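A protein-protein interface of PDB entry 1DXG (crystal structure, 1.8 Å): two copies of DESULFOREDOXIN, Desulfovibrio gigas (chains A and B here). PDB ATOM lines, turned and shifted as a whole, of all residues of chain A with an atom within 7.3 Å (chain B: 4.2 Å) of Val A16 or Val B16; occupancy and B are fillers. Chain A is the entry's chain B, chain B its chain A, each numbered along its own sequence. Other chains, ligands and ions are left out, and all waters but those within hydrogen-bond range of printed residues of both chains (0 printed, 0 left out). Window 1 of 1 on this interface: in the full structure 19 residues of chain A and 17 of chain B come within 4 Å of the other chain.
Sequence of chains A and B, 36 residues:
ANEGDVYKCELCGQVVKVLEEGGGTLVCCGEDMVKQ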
ATOM      1  N   ALA A   1     -21.183 -30.674  -5.786  1.00  0.00           N
ATOM      2  CA  ALA A   1     -20.070 -30.369  -4.899  1.00  0.00           C
ATOM      3  C   ALA A   1     -20.487 -30.639  -3.459  1.00  0.00           C
ATOM      4  O   ALA A   1     -21.675 -30.887  -3.245  1.00  0.00           O
ATOM      5  CB  ALA A   1     -19.703 -28.910  -5.028  1.00  0.00           C
ATOM      6  N   GLY A   4     -19.820 -26.565   2.376  1.00  0.00           N
ATOM      7  CA  GLY A   4     -18.651 -25.846   2.823  1.00  0.00           C
ATOM      8  C   GLY A   4     -17.666 -25.609   1.682  1.00  0.00           C
ATOM      9  O   GLY A   4     -16.779 -24.765   1.826  1.00  0.00           O
ATOM     10  N   ASP A   5     -17.734 -26.310   0.541  1.00  0.00           N
ATOM     11  CA  ASP A   5     -16.817 -26.050  -0.570  1.00  0.00           C
ATOM     12  C   ASP A   5     -17.013 -24.676  -1.177  1.00  0.00           C
ATOM     13  O   ASP A   5     -18.136 -24.177  -1.243  1.00  0.00           O
ATOM     14  CB  ASP A   5     -16.999 -27.056  -1.666  1.00  0.00           C
ATOM     15  CG  ASP A   5     -16.409 -28.429  -1.373  1.00  0.00           C
ATOM     16  OD1 ASP A   5     -15.608 -28.584  -0.445  1.00  0.00           O
ATOM     17  OD2 ASP A   5     -16.779 -29.353  -2.089  1.00  0.00           O
ATOM     18  N   VAL A   6     -15.901 -24.072  -1.590  1.00  0.00           N
ATOM     19  CA  VAL A   6     -15.903 -22.755  -2.181  1.00  0.00           C
ATOM     20  C   VAL A   6     -15.520 -22.923  -3.645  1.00  0.00           C
ATOM     21  O   VAL A   6     -14.512 -23.566  -3.935  1.00  0.00           O
ATOM     22  CB  VAL A   6     -14.891 -21.869  -1.413  1.00  0.00           C
ATOM     23  CG1 VAL A   6     -14.696 -20.534  -2.110  1.00  0.00           C
ATOM     24  CG2 VAL A   6     -15.441 -21.592  -0.009  1.00  0.00           C
ATOM     25  N   TYR A   7     -16.284 -22.375  -4.579  1.00  0.00           N
ATOM     26  CA  TYR A   7     -15.996 -22.460  -6.004  1.00  0.00           C
ATOM     27  C   TYR A   7     -15.912 -21.077  -6.615  1.00  0.00           C
ATOM     28  O   TYR A   7     -16.683 -20.190  -6.236  1.00  0.00           O
ATOM     29  CB  TYR A   7     -17.076 -23.205  -6.743  1.00  0.00           C
ATOM     30  CG  TYR A   7     -16.915 -24.706  -6.621  1.00  0.00           C
ATOM     31  CD1 TYR A   7     -17.206 -25.359  -5.406  1.00  0.00           C
ATOM     32  CD2 TYR A   7     -16.482 -25.426  -7.746  1.00  0.00           C
ATOM     33  CE1 TYR A   7     -17.023 -26.737  -5.307  1.00  0.00           C
ATOM     34  CE2 TYR A   7     -16.315 -26.805  -7.636  1.00  0.00           C
ATOM     35  CZ  TYR A   7     -16.570 -27.440  -6.419  1.00  0.00           C
ATOM     36  OH  TYR A   7     -16.392 -28.809  -6.357  1.00  0.00           O
ATOM     37  N   LYS A   8     -14.999 -20.873  -7.569  1.00  0.00           N
ATOM     38  CA  LYS A   8     -14.831 -19.589  -8.222  1.00  0.00           C
ATOM     39  C   LYS A   8     -14.988 -19.685  -9.729  1.00  0.00           C
ATOM     40  O   LYS A   8     -14.542 -20.667 -10.329  1.00  0.00           O
ATOM     41  CB  LYS A   8     -13.440 -19.021  -7.936  1.00  0.00           C
ATOM     42  CG  LYS A   8     -13.262 -17.625  -8.499  1.00  0.00           C
ATOM     43  CD  LYS A   8     -11.791 -17.290  -8.572  1.00  0.00           C
ATOM     44  CE  LYS A   8     -11.711 -15.888  -9.130  1.00  0.00           C
ATOM     45  NZ  LYS A   8     -10.358 -15.532  -9.492  1.00  0.00           N
ATOM     46  N   CYS A   9     -15.644 -18.728 -10.361  1.00  0.00           N
ATOM     47  CA  CYS A   9     -15.632 -18.649 -11.802  1.00  0.00           C
ATOM     48  C   CYS A   9     -14.411 -17.797 -12.160  1.00  0.00           C
ATOM     49  O   CYS A   9     -14.340 -16.606 -11.833  1.00  0.00           O
ATOM     50  CB  CYS A   9     -16.883 -17.972 -12.330  1.00  0.00           C
ATOM     51  SG  CYS A   9     -16.884 -17.707 -14.134  1.00  0.00           S
ATOM     52  N   GLY A  13     -15.158 -13.853 -11.993  1.00  0.00           N
ATOM     53  CA  GLY A  13     -14.807 -13.675 -10.606  1.00  0.00           C
ATOM     54  C   GLY A  13     -15.888 -14.065  -9.629  1.00  0.00           C
ATOM     55  O   GLY A  13     -15.671 -13.868  -8.436  1.00  0.00           O
ATOM     56  N   GLN A  14     -17.022 -14.655 -10.002  1.00  0.00           N
ATOM     57  CA  GLN A  14     -18.106 -14.910  -9.057  1.00  0.00           C
ATOM     58  C   GLN A  14     -17.666 -16.022  -8.125  1.00  0.00           C
ATOM     59  O   GLN A  14     -17.093 -16.993  -8.622  1.00  0.00           O
ATOM     60  CB  GLN A  14     -19.384 -15.328  -9.792  1.00  0.00           C
ATOM     61  CG  GLN A  14     -20.621 -15.502  -8.905  1.00  0.00           C
ATOM     62  CD  GLN A  14     -21.932 -15.262  -9.640  1.00  0.00           C
ATOM     63  OE1 GLN A  14     -22.756 -14.460  -9.204  1.00  0.00           O
ATOM     64  NE2 GLN A  14     -22.212 -15.840 -10.796  1.00  0.00           N
ATOM     65  N   VAL A  15     -17.876 -15.927  -6.819  1.00  0.00           N
ATOM     66  CA  VAL A  15     -17.441 -16.977  -5.896  1.00  0.00           C
ATOM     67  C   VAL A  15     -18.666 -17.439  -5.122  1.00  0.00           C
ATOM     68  O   VAL A  15     -19.418 -16.614  -4.588  1.00  0.00           O
ATOM     69  CB  VAL A  15     -16.366 -16.442  -4.903  1.00  0.00           C
ATOM     70  CG1 VAL A  15     -15.982 -17.510  -3.881  1.00  0.00           C
ATOM     71  CG2 VAL A  15     -15.114 -16.029  -5.681  1.00  0.00           C
ATOM     72  N   VAL A  16     -18.889 -18.741  -5.032  1.00  0.00           N
ATOM     73  CA  VAL A  16     -20.011 -19.283  -4.282  1.00  0.00           C
ATOM     74  C   VAL A  16     -19.513 -20.287  -3.255  1.00  0.00           C
ATOM     75  O   VAL A  16     -18.429 -20.859  -3.386  1.00  0.00           O
ATOM     76  CB  VAL A  16     -21.076 -19.997  -5.204  1.00  0.00           C
ATOM     77  CG1 VAL A  16     -21.653 -18.951  -6.171  1.00  0.00           C
ATOM     78  CG2 VAL A  16     -20.481 -21.202  -5.949  1.00  0.00           C
ATOM     79  N   LYS A  17     -20.282 -20.473  -2.200  1.00  0.00           N
ATOM     80  CA  LYS A  17     -19.984 -21.471  -1.194  1.00  0.00           C
ATOM     81  C   LYS A  17     -21.166 -22.417  -1.179  1.00  0.00           C
ATOM     82  O   LYS A  17     -22.317 -21.958  -1.198  1.00  0.00           O
ATOM     83  CB  LYS A  17     -19.831 -20.826   0.172  1.00  0.00           C
ATOM     84  CG  LYS A  17     -19.452 -21.807   1.285  1.00  0.00           C
ATOM     85  CD  LYS A  17     -19.197 -20.957   2.529  1.00  0.00           C
ATOM     86  CE  LYS A  17     -18.753 -21.785   3.703  1.00  0.00           C
ATOM     87  NZ  LYS A  17     -18.519 -20.914   4.859  1.00  0.00           N
ATOM     88  N   VAL A  18     -20.918 -23.719  -1.162  1.00  0.00           N
ATOM     89  CA  VAL A  18     -21.969 -24.735  -1.147  1.00  0.00           C
ATOM     90  C   VAL A  18     -22.601 -24.850   0.237  1.00  0.00           C
ATOM     91  O   VAL A  18     -21.893 -25.121   1.213  1.00  0.00           O
ATOM     92  CB  VAL A  18     -21.397 -26.126  -1.577  1.00  0.00           C
ATOM     93  CG1 VAL A  18     -22.481 -27.205  -1.549  1.00  0.00           C
ATOM     94  CG2 VAL A  18     -20.845 -26.025  -3.000  1.00  0.00           C
ATOM     95  N   LEU A  19     -23.920 -24.686   0.332  1.00  0.00           N
ATOM     96  CA  LEU A  19     -24.669 -24.808   1.572  1.00  0.00           C
ATOM     97  C   LEU A  19     -25.330 -26.163   1.708  1.00  0.00           C
ATOM     98  O   LEU A  19     -25.457 -26.666   2.823  1.00  0.00           O
ATOM     99  CB  LEU A  19     -25.760 -23.750   1.673  1.00  0.00           C
ATOM    100  CG  LEU A  19     -25.285 -22.315   1.789  1.00  0.00           C
ATOM    101  CD1 LEU A  19     -26.505 -21.422   1.841  1.00  0.00           C
ATOM    102  CD2 LEU A  19     -24.386 -22.151   3.008  1.00  0.00           C
ATOM    103  N   GLU A  20     -25.798 -26.753   0.614  1.00  0.00           N
ATOM    104  CA  GLU A  20     -26.418 -28.069   0.603  1.00  0.00           C
ATOM    105  C   GLU A  20     -25.845 -28.736  -0.628  1.00  0.00           C
ATOM    106  O   GLU A  20     -25.865 -28.146  -1.708  1.00  0.00           O
ATOM    107  CB  GLU A  20     -27.928 -27.991   0.458  1.00  0.00           C
ATOM    108  CG  GLU A  20     -28.649 -27.958   1.795  1.00  0.00           C
ATOM    109  CD  GLU A  20     -30.158 -27.802   1.650  1.00  0.00           C
ATOM    110  OE1 GLU A  20     -30.802 -28.686   1.086  1.00  0.00           O
ATOM    111  OE2 GLU A  20     -30.695 -26.789   2.092  1.00  0.00           O
ATOM    112  N   LEU A  26     -21.228 -27.334 -10.820  1.00  0.00           N
ATOM    113  CA  LEU A  26     -21.502 -25.902 -10.840  1.00  0.00           C
ATOM    114  C   LEU A  26     -20.840 -25.275 -12.056  1.00  0.00           C
ATOM    115  O   LEU A  26     -19.635 -25.462 -12.290  1.00  0.00           O
ATOM    116  CB  LEU A  26     -20.975 -25.274  -9.551  1.00  0.00           C
ATOM    117  CG  LEU A  26     -21.715 -25.702  -8.273  1.00  0.00           C
ATOM    118  CD1 LEU A  26     -21.001 -25.103  -7.075  1.00  0.00           C
ATOM    119  CD2 LEU A  26     -23.182 -25.273  -8.342  1.00  0.00           C
ATOM    120  N   MET A  33     -16.962 -24.148 -12.707  1.00  0.00           N
ATOM    121  CA  MET A  33     -16.361 -23.356 -11.642  1.00  0.00           C
ATOM    122  C   MET A  33     -15.232 -24.180 -10.998  1.00  0.00           C
ATOM    123  O   MET A  33     -15.239 -25.426 -10.985  1.00  0.00           O
ATOM    124  CB  MET A  33     -17.431 -22.999 -10.609  1.00  0.00           C
ATOM    125  CG  MET A  33     -18.487 -22.085 -11.216  1.00  0.00           C
ATOM    126  SD  MET A  33     -19.695 -21.539  -9.980  1.00  0.00           S
ATOM    127  CE  MET A  33     -18.860 -20.130  -9.292  1.00  0.00           C
ATOM    128  N   VAL A  34     -14.204 -23.484 -10.527  1.00  0.00           N
ATOM    129  CA  VAL A  34     -13.007 -24.128  -9.999  1.00  0.00           C
ATOM    130  C   VAL A  34     -13.050 -24.163  -8.476  1.00  0.00           C
ATOM    131  O   VAL A  34     -13.207 -23.109  -7.843  1.00  0.00           O
ATOM    132  CB  VAL A  34     -11.748 -23.342 -10.510  1.00  0.00           C
ATOM    133  CG1 VAL A  34     -10.454 -23.977  -9.971  1.00  0.00           C
ATOM    134  CG2 VAL A  34     -11.752 -23.323 -12.053  1.00  0.00           C
ATOM    135  N   GLN A  36     -11.828 -23.991  -4.783  1.00  0.00           N
ATOM    136  CA  GLN A  36     -10.730 -23.269  -4.157  1.00  0.00           C
ATOM    137  C   GLN A  36     -10.259 -24.028  -2.912  1.00  0.00           C
ATOM    138  O   GLN A  36     -11.085 -24.635  -2.245  1.00  0.00           O
ATOM    139  CB  GLN A  36     -11.209 -21.850  -3.792  1.00  0.00           C
ATOM    140  CG  GLN A  36     -11.669 -21.053  -5.030  1.00  0.00           C
ATOM    141  CD  GLN A  36     -10.560 -20.810  -6.056  1.00  0.00           C
ATOM    142  OE1 GLN A  36      -9.546 -20.185  -5.730  1.00  0.00           O
ATOM    143  NE2 GLN A  36     -10.663 -21.277  -7.291  1.00  0.00           N
ATOM    144  OXT GLN A  36      -9.066 -24.058  -2.624  1.00  0.00           O
ATOM    145  N   ASP B   5     -26.821 -13.476  -1.984  1.00  0.00           N
ATOM    146  CA  ASP B   5     -27.940 -14.221  -2.557  1.00  0.00           C
ATOM    147  C   ASP B   5     -27.722 -15.725  -2.441  1.00  0.00           C
ATOM    148  O   ASP B   5     -26.581 -16.197  -2.459  1.00  0.00           O
ATOM    149  CB  ASP B   5     -28.125 -13.910  -4.029  1.00  0.00           C
ATOM    150  CG  ASP B   5     -28.720 -12.551  -4.316  1.00  0.00           C
ATOM    151  OD1 ASP B   5     -29.352 -11.958  -3.436  1.00  0.00           O
ATOM    152  OD2 ASP B   5     -28.536 -12.092  -5.445  1.00  0.00           O
ATOM    153  N   VAL B   6     -28.796 -16.490  -2.378  1.00  0.00           N
ATOM    154  CA  VAL B   6     -28.738 -17.930  -2.265  1.00  0.00           C
ATOM    155  C   VAL B   6     -29.400 -18.451  -3.529  1.00  0.00           C
ATOM    156  O   VAL B   6     -30.469 -17.967  -3.914  1.00  0.00           O
ATOM    157  CB  VAL B   6     -29.500 -18.364  -0.987  1.00  0.00           C
ATOM    158  CG1 VAL B   6     -29.646 -19.883  -0.942  1.00  0.00           C
ATOM    159  CG2 VAL B   6     -28.724 -17.898   0.245  1.00  0.00           C
ATOM    160  N   TYR B   7     -28.805 -19.434  -4.193  1.00  0.00           N
ATOM    161  CA  TYR B   7     -29.342 -20.010  -5.410  1.00  0.00           C
ATOM    162  C   TYR B   7     -29.486 -21.509  -5.233  1.00  0.00           C
ATOM    163  O   TYR B   7     -28.627 -22.163  -4.627  1.00  0.00           O
ATOM    164  CB  TYR B   7     -28.422 -19.730  -6.572  1.00  0.00           C
ATOM    165  CG  TYR B   7     -28.661 -18.358  -7.176  1.00  0.00           C
ATOM    166  CD1 TYR B   7     -28.131 -17.195  -6.577  1.00  0.00           C
ATOM    167  CD2 TYR B   7     -29.436 -18.279  -8.337  1.00  0.00           C
ATOM    168  CE1 TYR B   7     -28.409 -15.955  -7.145  1.00  0.00           C
ATOM    169  CE2 TYR B   7     -29.699 -17.031  -8.895  1.00  0.00           C
ATOM    170  CZ  TYR B   7     -29.193 -15.888  -8.296  1.00  0.00           C
ATOM    171  OH  TYR B   7     -29.462 -14.677  -8.894  1.00  0.00           O
ATOM    172  N   VAL B  15     -27.547 -26.191  -3.122  1.00  0.00           N
ATOM    173  CA  VAL B  15     -27.832 -24.812  -2.749  1.00  0.00           C
ATOM    174  C   VAL B  15     -26.509 -24.107  -2.566  1.00  0.00           C
ATOM    175  O   VAL B  15     -25.668 -24.647  -1.842  1.00  0.00           O
ATOM    176  CB  VAL B  15     -28.638 -24.728  -1.413  1.00  0.00           C
ATOM    177  CG1 VAL B  15     -28.993 -23.288  -1.110  1.00  0.00           C
ATOM    178  CG2 VAL B  15     -29.956 -25.449  -1.523  1.00  0.00           C
ATOM    179  N   VAL B  16     -26.277 -22.937  -3.154  1.00  0.00           N
ATOM    180  CA  VAL B  16     -25.049 -22.200  -2.918  1.00  0.00           C
ATOM    181  C   VAL B  16     -25.370 -20.780  -2.484  1.00  0.00           C
ATOM    182  O   VAL B  16     -26.463 -20.273  -2.760  1.00  0.00           O
ATOM    183  CB  VAL B  16     -24.118 -22.120  -4.182  1.00  0.00           C
ATOM    184  CG1 VAL B  16     -23.742 -23.544  -4.601  1.00  0.00           C
ATOM    185  CG2 VAL B  16     -24.775 -21.345  -5.340  1.00  0.00           C
ATOM    186  N   LYS B  17     -24.448 -20.145  -1.779  1.00  0.00           N
ATOM    187  CA  LYS B  17     -24.548 -18.742  -1.362  1.00  0.00           C
ATOM    188  C   LYS B  17     -23.518 -17.952  -2.153  1.00  0.00           C
ATOM    189  O   LYS B  17     -22.377 -18.412  -2.271  1.00  0.00           O
ATOM    190  CB  LYS B  17     -24.223 -18.601   0.114  1.00  0.00           C
ATOM    191  CG  LYS B  17     -24.112 -17.168   0.684  1.00  0.00           C
ATOM    192  CD  LYS B  17     -23.142 -17.293   1.862  1.00  0.00           C
ATOM    193  CE  LYS B  17     -23.657 -16.628   3.121  1.00  0.00           C
ATOM    194  NZ  LYS B  17     -23.503 -15.189   3.115  1.00  0.00           N
ATOM    195  N   LEU B  26     -25.321 -18.772 -12.987  1.00  0.00           N
ATOM    196  CA  LEU B  26     -25.012 -20.014 -12.306  1.00  0.00           C
ATOM    197  C   LEU B  26     -25.886 -21.105 -12.885  1.00  0.00           C
ATOM    198  O   LEU B  26     -27.114 -20.974 -12.933  1.00  0.00           O
ATOM    199  CB  LEU B  26     -25.281 -19.875 -10.826  1.00  0.00           C
ATOM    200  CG  LEU B  26     -24.380 -18.894 -10.073  1.00  0.00           C
ATOM    201  CD1 LEU B  26     -24.920 -18.733  -8.668  1.00  0.00           C
ATOM    202  CD2 LEU B  26     -22.942 -19.383 -10.083  1.00  0.00           C
ATOM    203  N   MET B  33     -29.765 -21.961 -12.139  1.00  0.00           N
ATOM    204  CA  MET B  33     -30.121 -22.062 -10.733  1.00  0.00           C
ATOM    205  C   MET B  33     -31.126 -20.958 -10.393  1.00  0.00           C
ATOM    206  O   MET B  33     -31.181 -19.927 -11.054  1.00  0.00           O
ATOM    207  CB  MET B  33     -28.861 -21.950  -9.876  1.00  0.00           C
ATOM    208  CG  MET B  33     -28.009 -23.226  -9.972  1.00  0.00           C
ATOM    209  SD  MET B  33     -26.481 -23.175  -9.002  1.00  0.00           S
ATOM    210  CE  MET B  33     -27.073 -23.893  -7.495  1.00  0.00           C
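The backbone carbonyl oxygen of Val B15 sits at hydrogen-bond distance from the backbone NH of Leu A19.
The backbone NH of Val B15 is in hydrogen-bond range of the backbone carbonyl oxygen of Glu A20.
The backbone carbonyl oxygen (O) of Lys A17 sits at hydrogen-bond distance from the backbone NH (N) of Lys B17, 2.9 Å away.
Of the 19 printed residues of chain A, 8 touch a printed residue of chain B.
Hydrophobic or aromatic side chains of chain A within 4 Å of the printed part of chain B: Val A16, Leu A19, Leu A26 and Met A33.
Of the 8 printed residues of chain B, 5 touch a printed residue of chain A.
Among the printed residues, no Asp or Glu carboxylate lies within 4 Å of a Lys or Arg side-chain nitrogen of the other chain.
NE2 of Gln A14 touches CD2 of Leu B26, at 3.7 Å.
Val B16 touches Val A16 (CB to CB, 3.8 Å).
CA of Val A16 touches O of Lys B17 (3.2 Å).
Lys A17 touches Val B16.
Val A18 touches Val B15 (C to O, 3.7 Å).
Leu A26 touches Met B33 (CD2 to SD, 3.96 Å).
Met A33 touches Leu B26.
Ala A1 touches none of the printed residues of chain B.
Printed residues of chain B within 4 Å of Gln A14: Leu B26.
Of chain B, only Val B16 and Lys B17 come within 4 Å of Val A16.
Of the printed residues of chain B, Glu A20 touches Val B15.
Printed residues of chain B within 4 Å of Leu A26: Met B33.
Of the printed residues of chain A, Val B15 touches Val A18 (3.7 Å), Leu A19 (2.8 Å) and Glu A20 (2.9 Å).
Of the printed residues of chain A, Val B16 touches Val A16 (3.8 Å) and Lys A17 (3.2 Å).
Printed residues of chain A within 4 Å of Lys B17: Val A16 and Lys A17.
Val A16 touches its own counterpart, Val B16.
Val A16 touches Lys B17, and with the chains exchanged Lys A17 touches Val B16.
Lys A17 touches its own counterpart, Lys B17.
Leu A26 touches Met B33, and with the chains exchanged Met A33 touches Leu B26.
Positions printed for both chains: 5, 6, 7, 15, 16, 17, 26 and 33.
N of Tyr B7 lies within hydrogen-bond range of O of Val B16.
N of Gly A4 sits at hydrogen-bond distance from O of Val A18, at 2.8 Å.
The backbone carbonyl oxygen of Asp A5 sits at hydrogen-bond distance from the backbone NH of Val A18, at 2.8 Å.
The backbone NH (N) of Tyr A7 is in hydrogen-bond range of the backbone carbonyl oxygen (O) of Val A16 (2.9 Å).
O of Gln A14 is in hydrogen-bond range of N of Cys A9 (2.9 Å).
The backbone NH (N) of Met A33 lies within hydrogen-bond range of the backbone carbonyl oxygen (O) of Leu A26 (3.0 Å).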
